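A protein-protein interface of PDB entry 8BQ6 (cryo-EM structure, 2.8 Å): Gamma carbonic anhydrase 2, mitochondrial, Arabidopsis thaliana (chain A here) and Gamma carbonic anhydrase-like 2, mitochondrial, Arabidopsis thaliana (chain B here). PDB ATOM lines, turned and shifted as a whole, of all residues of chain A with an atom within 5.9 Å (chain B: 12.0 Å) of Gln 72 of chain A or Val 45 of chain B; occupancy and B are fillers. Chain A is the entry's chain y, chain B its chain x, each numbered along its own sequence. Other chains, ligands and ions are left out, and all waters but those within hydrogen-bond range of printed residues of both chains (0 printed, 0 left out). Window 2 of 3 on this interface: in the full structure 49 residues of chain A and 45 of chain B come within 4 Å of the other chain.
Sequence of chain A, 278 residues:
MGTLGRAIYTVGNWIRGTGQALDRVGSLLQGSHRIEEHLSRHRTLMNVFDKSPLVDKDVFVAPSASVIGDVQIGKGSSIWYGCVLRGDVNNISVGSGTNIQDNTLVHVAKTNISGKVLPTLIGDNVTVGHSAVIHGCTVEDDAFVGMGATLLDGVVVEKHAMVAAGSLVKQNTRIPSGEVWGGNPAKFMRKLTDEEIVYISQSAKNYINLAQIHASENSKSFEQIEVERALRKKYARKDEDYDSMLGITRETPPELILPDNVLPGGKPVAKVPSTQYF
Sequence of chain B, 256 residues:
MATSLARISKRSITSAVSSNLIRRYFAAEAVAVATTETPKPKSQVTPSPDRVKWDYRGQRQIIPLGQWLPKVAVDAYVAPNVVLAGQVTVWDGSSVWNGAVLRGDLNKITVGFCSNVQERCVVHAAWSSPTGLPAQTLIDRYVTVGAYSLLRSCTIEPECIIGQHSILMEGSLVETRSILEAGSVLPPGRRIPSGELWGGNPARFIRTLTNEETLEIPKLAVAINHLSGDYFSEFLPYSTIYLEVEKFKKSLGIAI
The side-chain carboxylate of Asp 56 of chain A sits at hydrogen-bond distance from the backbone NH of Thr 46 of chain B (2.7 Å).
NH2 of Arg 51 of chain B sits at hydrogen-bond distance from O of Asp 56 of chain A (3.0 Å).
Of chain A, only Leu 54 (3.8 Å), Val 55 (3.9 Å), Asp 56 (3.3 Å), Gln 72 (3.2 Å), Ile 73 (3.3 Å) and Gly 74 (3.9 Å) come within 4 Å of Val 45 of chain B.
Pro 53 of chain A touches none of the printed residues of chain B.
Asp 56 of chain A touches four residues of chain B.
No residue of chain B comes within 4 Å of Asp 70 of chain A.
No residue of chain B comes within 4 Å of Val 71 of chain A.
Printed residues of chain B within 4 Å of Ile 73 of chain A: Val 45 (3.3 Å).
Of chain B, only Val 45 comes within 4 Å of Gly 74 of chain A.
No residue of chain B comes within 4 Å of Ile 92 of chain A.
No residue of chain B comes within 4 Å of Gly 95 of chain A.
Printed residues of chain A within 4 Å of Thr 46 of chain B: Asp 56.
Of the printed residues of chain A, Pro 47 of chain B touches Val 55.
The nearest residue of chain B that does not touch Gln 72 of chain A is Gln 44 of chain B (5.8 Å).
The nearest printed residue of chain A that does not touch Gln 44 of chain B is Lys 75 of chain A (4.9 Å).
CG1 of Val 45 of chain B touches O of Leu 54 of chain A, 3.8 Å away.
Val 45 of chain B touches Val 55 of chain A (CG1 to C, 3.9 Å).
Val 55 of chain A touches Pro 47 of chain B (O to CA, 3.1 Å).
Val 55 of chain A touches Arg 51 of chain B (CG1 to NE, 3.9 Å).
Asp 56 of chain A touches Gln 44 of chain B (OD1 to O, 3.5 Å).
Val 45 of chain B touches Asp 56 of chain A.
CG2 of Val 45 of chain B touches NE2 of Gln 72 of chain A, at 3.2 Å.
Val 45 of chain B touches Ile 73 of chain A (CG1 to O, 3.3 Å).
Gly 74 of chain A touches Val 45 of chain B.
The backbone NH of Arg 51 of chain B lies close to the side-chain hydroxyl of Ser 48 of chain B (3.1 Å).
O of Val 71 of chain A is in hydrogen-bond range of N of Leu 54 of chain A (2.7 Å).
The backbone NH (N) of Asp 56 of chain A sits at hydrogen-bond distance from the backbone carbonyl oxygen (O) of Ile 73 of chain A, at 3.2 Å.
The backbone carbonyl oxygen (O) of Gln 72 of chain A lies within hydrogen-bond range of the backbone NH (N) of Val 94 of chain A.
N of Gly 74 of chain A sits at hydrogen-bond distance from O of Val 94 of chain A (3.0 Å).
The backbone carbonyl oxygen (O) of Gly 95 of chain A is in hydrogen-bond range of the backbone NH (N) of Gly 74 of chain A (3.5 Å).
Of the 8 printed residues of chain B, 5 touch a printed residue of chain A.
Of the 15 printed residues of chain A, 6 touch a printed residue of chain B.
Among the printed residues, 11 pairs touch across the chains.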
ATOM      1  N   PRO A  53      -8.827  -8.385 -23.475  1.00  0.00           N
ATOM      2  CA  PRO A  53     -10.097  -8.923 -22.975  1.00  0.00           C
ATOM      3  C   PRO A  53      -9.931 -10.307 -22.362  1.00  0.00           C
ATOM      4  O   PRO A  53      -9.191 -11.152 -22.868  1.00  0.00           O
ATOM      5  CB  PRO A  53     -10.990  -8.954 -24.221  1.00  0.00           C
ATOM      6  CG  PRO A  53     -10.077  -8.828 -25.372  1.00  0.00           C
ATOM      7  CD  PRO A  53      -8.878  -8.079 -24.913  1.00  0.00           C
ATOM      8  N   LEU A  54     -10.633 -10.524 -21.254  1.00  0.00           N
ATOM      9  CA  LEU A  54     -10.619 -11.782 -20.512  1.00  0.00           C
ATOM     10  C   LEU A  54     -11.950 -12.481 -20.765  1.00  0.00           C
ATOM     11  O   LEU A  54     -12.982 -12.085 -20.218  1.00  0.00           O
ATOM     12  CB  LEU A  54     -10.398 -11.528 -19.026  1.00  0.00           C
ATOM     13  CG  LEU A  54     -10.210 -12.753 -18.132  1.00  0.00           C
ATOM     14  CD1 LEU A  54      -8.956 -13.524 -18.519  1.00  0.00           C
ATOM     15  CD2 LEU A  54     -10.166 -12.340 -16.672  1.00  0.00           C
ATOM     16  N   VAL A  55     -11.924 -13.522 -21.587  1.00  0.00           N
ATOM     17  CA  VAL A  55     -13.133 -14.159 -22.090  1.00  0.00           C
ATOM     18  C   VAL A  55     -13.094 -15.627 -21.700  1.00  0.00           C
ATOM     19  O   VAL A  55     -12.073 -16.295 -21.891  1.00  0.00           O
ATOM     20  CB  VAL A  55     -13.255 -14.000 -23.615  1.00  0.00           C
ATOM     21  CG1 VAL A  55     -14.586 -14.531 -24.102  1.00  0.00           C
ATOM     22  CG2 VAL A  55     -13.072 -12.550 -24.008  1.00  0.00           C
ATOM     23  N   ASP A  56     -14.199 -16.127 -21.156  1.00  0.00           N
ATOM     24  CA  ASP A  56     -14.230 -17.501 -20.682  1.00  0.00           C
ATOM     25  C   ASP A  56     -14.191 -18.486 -21.848  1.00  0.00           C
ATOM     26  O   ASP A  56     -14.409 -18.133 -23.011  1.00  0.00           O
ATOM     27  CB  ASP A  56     -15.480 -17.750 -19.836  1.00  0.00           C
ATOM     28  CG  ASP A  56     -15.362 -18.998 -18.981  1.00  0.00           C
ATOM     29  OD1 ASP A  56     -14.842 -18.897 -17.852  1.00  0.00           O
ATOM     30  OD2 ASP A  56     -15.777 -20.083 -19.438  1.00  0.00           O
ATOM     31  N   ASP A  70     -10.410  -3.608 -22.098  1.00  0.00           N
ATOM     32  CA  ASP A  70     -10.533  -4.214 -20.776  1.00  0.00           C
ATOM     33  C   ASP A  70     -11.960  -4.726 -20.602  1.00  0.00           C
ATOM     34  O   ASP A  70     -12.806  -4.112 -19.952  1.00  0.00           O
ATOM     35  CB  ASP A  70     -10.149  -3.204 -19.702  1.00  0.00           C
ATOM     36  CG  ASP A  70     -10.113  -3.808 -18.318  1.00  0.00           C
ATOM     37  OD1 ASP A  70     -10.145  -5.050 -18.204  1.00  0.00           O
ATOM     38  OD2 ASP A  70     -10.044  -3.039 -17.339  1.00  0.00           O
ATOM     39  N   VAL A  71     -12.219  -5.884 -21.202  1.00  0.00           N
ATOM     40  CA  VAL A  71     -13.536  -6.507 -21.196  1.00  0.00           C
ATOM     41  C   VAL A  71     -13.426  -7.864 -20.524  1.00  0.00           C
ATOM     42  O   VAL A  71     -12.528  -8.649 -20.844  1.00  0.00           O
ATOM     43  CB  VAL A  71     -14.103  -6.665 -22.620  1.00  0.00           C
ATOM     44  CG1 VAL A  71     -15.561  -7.058 -22.565  1.00  0.00           C
ATOM     45  CG2 VAL A  71     -13.933  -5.383 -23.401  1.00  0.00           C
ATOM     46  N   GLN A  72     -14.337  -8.140 -19.598  1.00  0.00           N
ATOM     47  CA  GLN A  72     -14.442  -9.444 -18.965  1.00  0.00           C
ATOM     48  C   GLN A  72     -15.812 -10.025 -19.270  1.00  0.00           C
ATOM     49  O   GLN A  72     -16.833  -9.378 -19.019  1.00  0.00           O
ATOM     50  CB  GLN A  72     -14.230  -9.349 -17.455  1.00  0.00           C
ATOM     51  CG  GLN A  72     -14.187 -10.698 -16.770  1.00  0.00           C
ATOM     52  CD  GLN A  72     -13.810 -10.601 -15.306  1.00  0.00           C
ATOM     53  OE1 GLN A  72     -13.486  -9.525 -14.805  1.00  0.00           O
ATOM     54  NE2 GLN A  72     -13.845 -11.732 -14.612  1.00  0.00           N
ATOM     55  N   ILE A  73     -15.828 -11.236 -19.818  1.00  0.00           N
ATOM     56  CA  ILE A  73     -17.058 -11.935 -20.165  1.00  0.00           C
ATOM     57  C   ILE A  73     -17.031 -13.288 -19.473  1.00  0.00           C
ATOM     58  O   ILE A  73     -16.053 -14.032 -19.600  1.00  0.00           O
ATOM     59  CB  ILE A  73     -17.204 -12.110 -21.688  1.00  0.00           C
ATOM     60  CG1 ILE A  73     -17.106 -10.765 -22.396  1.00  0.00           C
ATOM     61  CG2 ILE A  73     -18.523 -12.748 -22.029  1.00  0.00           C
ATOM     62  CD1 ILE A  73     -16.785 -10.903 -23.851  1.00  0.00           C
ATOM     63  N   GLY A  74     -18.104 -13.608 -18.749  1.00  0.00           N
ATOM     64  CA  GLY A  74     -18.142 -14.801 -17.932  1.00  0.00           C
ATOM     65  C   GLY A  74     -18.749 -16.005 -18.632  1.00  0.00           C
ATOM     66  O   GLY A  74     -19.196 -15.951 -19.776  1.00  0.00           O
ATOM     67  N   LYS A  75     -18.791 -17.106 -17.885  1.00  0.00           N
ATOM     68  CA  LYS A  75     -19.157 -18.408 -18.427  1.00  0.00           C
ATOM     69  C   LYS A  75     -20.570 -18.416 -19.004  1.00  0.00           C
ATOM     70  O   LYS A  75     -21.516 -17.922 -18.390  1.00  0.00           O
ATOM     71  CB  LYS A  75     -19.031 -19.454 -17.322  1.00  0.00           C
ATOM     72  CG  LYS A  75     -19.383 -20.854 -17.734  1.00  0.00           C
ATOM     73  CD  LYS A  75     -20.343 -21.466 -16.743  1.00  0.00           C
ATOM     74  CE  LYS A  75     -20.439 -22.963 -16.939  1.00  0.00           C
ATOM     75  NZ  LYS A  75     -21.733 -23.336 -17.571  1.00  0.00           N
ATOM     76  N   ASN A  91     -13.484  -0.064 -17.763  1.00  0.00           N
ATOM     77  CA  ASN A  91     -13.719  -1.500 -17.712  1.00  0.00           C
ATOM     78  C   ASN A  91     -15.144  -1.818 -18.147  1.00  0.00           C
ATOM     79  O   ASN A  91     -16.066  -1.035 -17.911  1.00  0.00           O
ATOM     80  CB  ASN A  91     -13.469  -2.027 -16.296  1.00  0.00           C
ATOM     81  CG  ASN A  91     -13.570  -3.539 -16.202  1.00  0.00           C
ATOM     82  OD1 ASN A  91     -13.208  -4.258 -17.130  1.00  0.00           O
ATOM     83  ND2 ASN A  91     -14.047  -4.027 -15.064  1.00  0.00           N
ATOM     84  N   ILE A  92     -15.311  -2.961 -18.811  1.00  0.00           N
ATOM     85  CA  ILE A  92     -16.621  -3.531 -19.104  1.00  0.00           C
ATOM     86  C   ILE A  92     -16.640  -4.944 -18.549  1.00  0.00           C
ATOM     87  O   ILE A  92     -15.772  -5.757 -18.887  1.00  0.00           O
ATOM     88  CB  ILE A  92     -16.931  -3.558 -20.609  1.00  0.00           C
ATOM     89  CG1 ILE A  92     -17.012  -2.151 -21.182  1.00  0.00           C
ATOM     90  CG2 ILE A  92     -18.248  -4.271 -20.857  1.00  0.00           C
ATOM     91  CD1 ILE A  92     -17.180  -2.146 -22.670  1.00  0.00           C
ATOM     92  N   SER A  93     -17.633  -5.242 -17.720  1.00  0.00           N
ATOM     93  CA  SER A  93     -17.762  -6.554 -17.106  1.00  0.00           C
ATOM     94  C   SER A  93     -19.093  -7.167 -17.505  1.00  0.00           C
ATOM     95  O   SER A  93     -20.139  -6.525 -17.375  1.00  0.00           O
ATOM     96  CB  SER A  93     -17.664  -6.463 -15.584  1.00  0.00           C
ATOM     97  OG  SER A  93     -16.328  -6.631 -15.154  1.00  0.00           O
ATOM     98  N   VAL A  94     -19.049  -8.404 -17.984  1.00  0.00           N
ATOM     99  CA  VAL A  94     -20.241  -9.150 -18.360  1.00  0.00           C
ATOM    100  C   VAL A  94     -20.289 -10.411 -17.514  1.00  0.00           C
ATOM    101  O   VAL A  94     -19.302 -11.153 -17.438  1.00  0.00           O
ATOM    102  CB  VAL A  94     -20.254  -9.484 -19.862  1.00  0.00           C
ATOM    103  CG1 VAL A  94     -21.364 -10.468 -20.180  1.00  0.00           C
ATOM    104  CG2 VAL A  94     -20.425  -8.209 -20.672  1.00  0.00           C
ATOM    105  N   GLY A  95     -21.429 -10.646 -16.875  1.00  0.00           N
ATOM    106  CA  GLY A  95     -21.569 -11.793 -16.005  1.00  0.00           C
ATOM    107  C   GLY A  95     -21.714 -13.093 -16.764  1.00  0.00           C
ATOM    108  O   GLY A  95     -21.462 -13.150 -17.970  1.00  0.00           O
ATOM    109  N   GLN B  44     -15.808 -17.700 -11.726  1.00  0.00           N
ATOM    110  CA  GLN B  44     -14.477 -17.519 -12.293  1.00  0.00           C
ATOM    111  C   GLN B  44     -14.527 -17.471 -13.813  1.00  0.00           C
ATOM    112  O   GLN B  44     -15.361 -18.127 -14.433  1.00  0.00           O
ATOM    113  CB  GLN B  44     -13.537 -18.642 -11.856  1.00  0.00           C
ATOM    114  CG  GLN B  44     -12.073 -18.289 -12.071  1.00  0.00           C
ATOM    115  CD  GLN B  44     -11.200 -19.488 -12.371  1.00  0.00           C
ATOM    116  OE1 GLN B  44     -11.602 -20.408 -13.083  1.00  0.00           O
ATOM    117  NE2 GLN B  44      -9.989 -19.479 -11.831  1.00  0.00           N
ATOM    118  N   VAL B  45     -13.619 -16.715 -14.415  1.00  0.00           N
ATOM    119  CA  VAL B  45     -13.534 -16.590 -15.864  1.00  0.00           C
ATOM    120  C   VAL B  45     -12.245 -17.279 -16.297  1.00  0.00           C
ATOM    121  O   VAL B  45     -11.158 -16.694 -16.217  1.00  0.00           O
ATOM    122  CB  VAL B  45     -13.569 -15.126 -16.315  1.00  0.00           C
ATOM    123  CG1 VAL B  45     -13.415 -15.033 -17.822  1.00  0.00           C
ATOM    124  CG2 VAL B  45     -14.859 -14.466 -15.863  1.00  0.00           C
ATOM    125  N   THR B  46     -12.355 -18.525 -16.761  1.00  0.00           N
ATOM    126  CA  THR B  46     -11.188 -19.256 -17.232  1.00  0.00           C
ATOM    127  C   THR B  46     -11.149 -19.256 -18.754  1.00  0.00           C
ATOM    128  O   THR B  46     -12.042 -19.836 -19.391  1.00  0.00           O
ATOM    129  CB  THR B  46     -11.174 -20.688 -16.683  1.00  0.00           C
ATOM    130  OG1 THR B  46     -10.174 -21.458 -17.365  1.00  0.00           O
ATOM    131  CG2 THR B  46     -12.542 -21.367 -16.788  1.00  0.00           C
ATOM    132  N   PRO B  47     -10.157 -18.624 -19.373  1.00  0.00           N
ATOM    133  CA  PRO B  47     -10.149 -18.484 -20.831  1.00  0.00           C
ATOM    134  C   PRO B  47      -9.603 -19.720 -21.535  1.00  0.00           C
ATOM    135  O   PRO B  47      -9.182 -20.699 -20.920  1.00  0.00           O
ATOM    136  CB  PRO B  47      -9.238 -17.273 -21.052  1.00  0.00           C
ATOM    137  CG  PRO B  47      -8.301 -17.309 -19.909  1.00  0.00           C
ATOM    138  CD  PRO B  47      -9.049 -17.892 -18.739  1.00  0.00           C
ATOM    139  N   SER B  48      -9.641 -19.650 -22.866  1.00  0.00           N
ATOM    140  CA  SER B  48      -9.120 -20.675 -23.752  1.00  0.00           C
ATOM    141  C   SER B  48      -7.906 -20.150 -24.494  1.00  0.00           C
ATOM    142  O   SER B  48      -7.979 -19.077 -25.107  1.00  0.00           O
ATOM    143  CB  SER B  48     -10.185 -21.118 -24.758  1.00  0.00           C
ATOM    144  OG  SER B  48     -10.379 -20.161 -25.775  1.00  0.00           O
ATOM    145  N   PRO B  49      -6.775 -20.858 -24.443  1.00  0.00           N
ATOM    146  CA  PRO B  49      -5.630 -20.469 -25.280  1.00  0.00           C
ATOM    147  C   PRO B  49      -5.849 -20.699 -26.765  1.00  0.00           C
ATOM    148  O   PRO B  49      -5.079 -20.162 -27.569  1.00  0.00           O
ATOM    149  CB  PRO B  49      -4.482 -21.339 -24.745  1.00  0.00           C
ATOM    150  CG  PRO B  49      -4.955 -21.860 -23.413  1.00  0.00           C
ATOM    151  CD  PRO B  49      -6.443 -21.953 -23.517  1.00  0.00           C
ATOM    152  N   ARG B  51      -8.707 -19.837 -28.390  1.00  0.00           N
ATOM    153  CA  ARG B  51      -9.719 -18.937 -28.927  1.00  0.00           C
ATOM    154  C   ARG B  51      -9.137 -18.101 -30.058  1.00  0.00           C
ATOM    155  O   ARG B  51      -8.051 -17.528 -29.934  1.00  0.00           O
ATOM    156  CB  ARG B  51     -10.265 -18.017 -27.840  1.00  0.00           C
ATOM    157  CG  ARG B  51     -11.130 -16.895 -28.377  1.00  0.00           C
ATOM    158  CD  ARG B  51     -11.897 -16.184 -27.278  1.00  0.00           C
ATOM    159  NE  ARG B  51     -12.747 -17.065 -26.485  1.00  0.00           N
ATOM    160  CZ  ARG B  51     -14.002 -17.371 -26.784  1.00  0.00           C
ATOM    161  NH1 ARG B  51     -14.582 -16.919 -27.883  1.00  0.00           N
ATOM    162  NH2 ARG B  51     -14.697 -18.140 -25.952  1.00  0.00           N
ATOM    163  N   LYS B  53      -8.618 -15.015 -32.165  1.00  0.00           N
ATOM    164  CA  LYS B  53      -8.735 -13.576 -31.980  1.00  0.00           C
ATOM    165  C   LYS B  53      -8.802 -12.827 -33.303  1.00  0.00           C
ATOM    166  O   LYS B  53      -9.543 -11.847 -33.420  1.00  0.00           O
ATOM    167  CB  LYS B  53      -7.564 -13.069 -31.141  1.00  0.00           C
ATOM    168  CG  LYS B  53      -7.600 -13.608 -29.733  1.00  0.00           C
ATOM    169  CD  LYS B  53      -6.510 -13.036 -28.865  1.00  0.00           C
ATOM    170  CE  LYS B  53      -6.562 -13.665 -27.481  1.00  0.00           C
ATOM    171  NZ  LYS B  53      -6.751 -15.145 -27.546  1.00  0.00           N
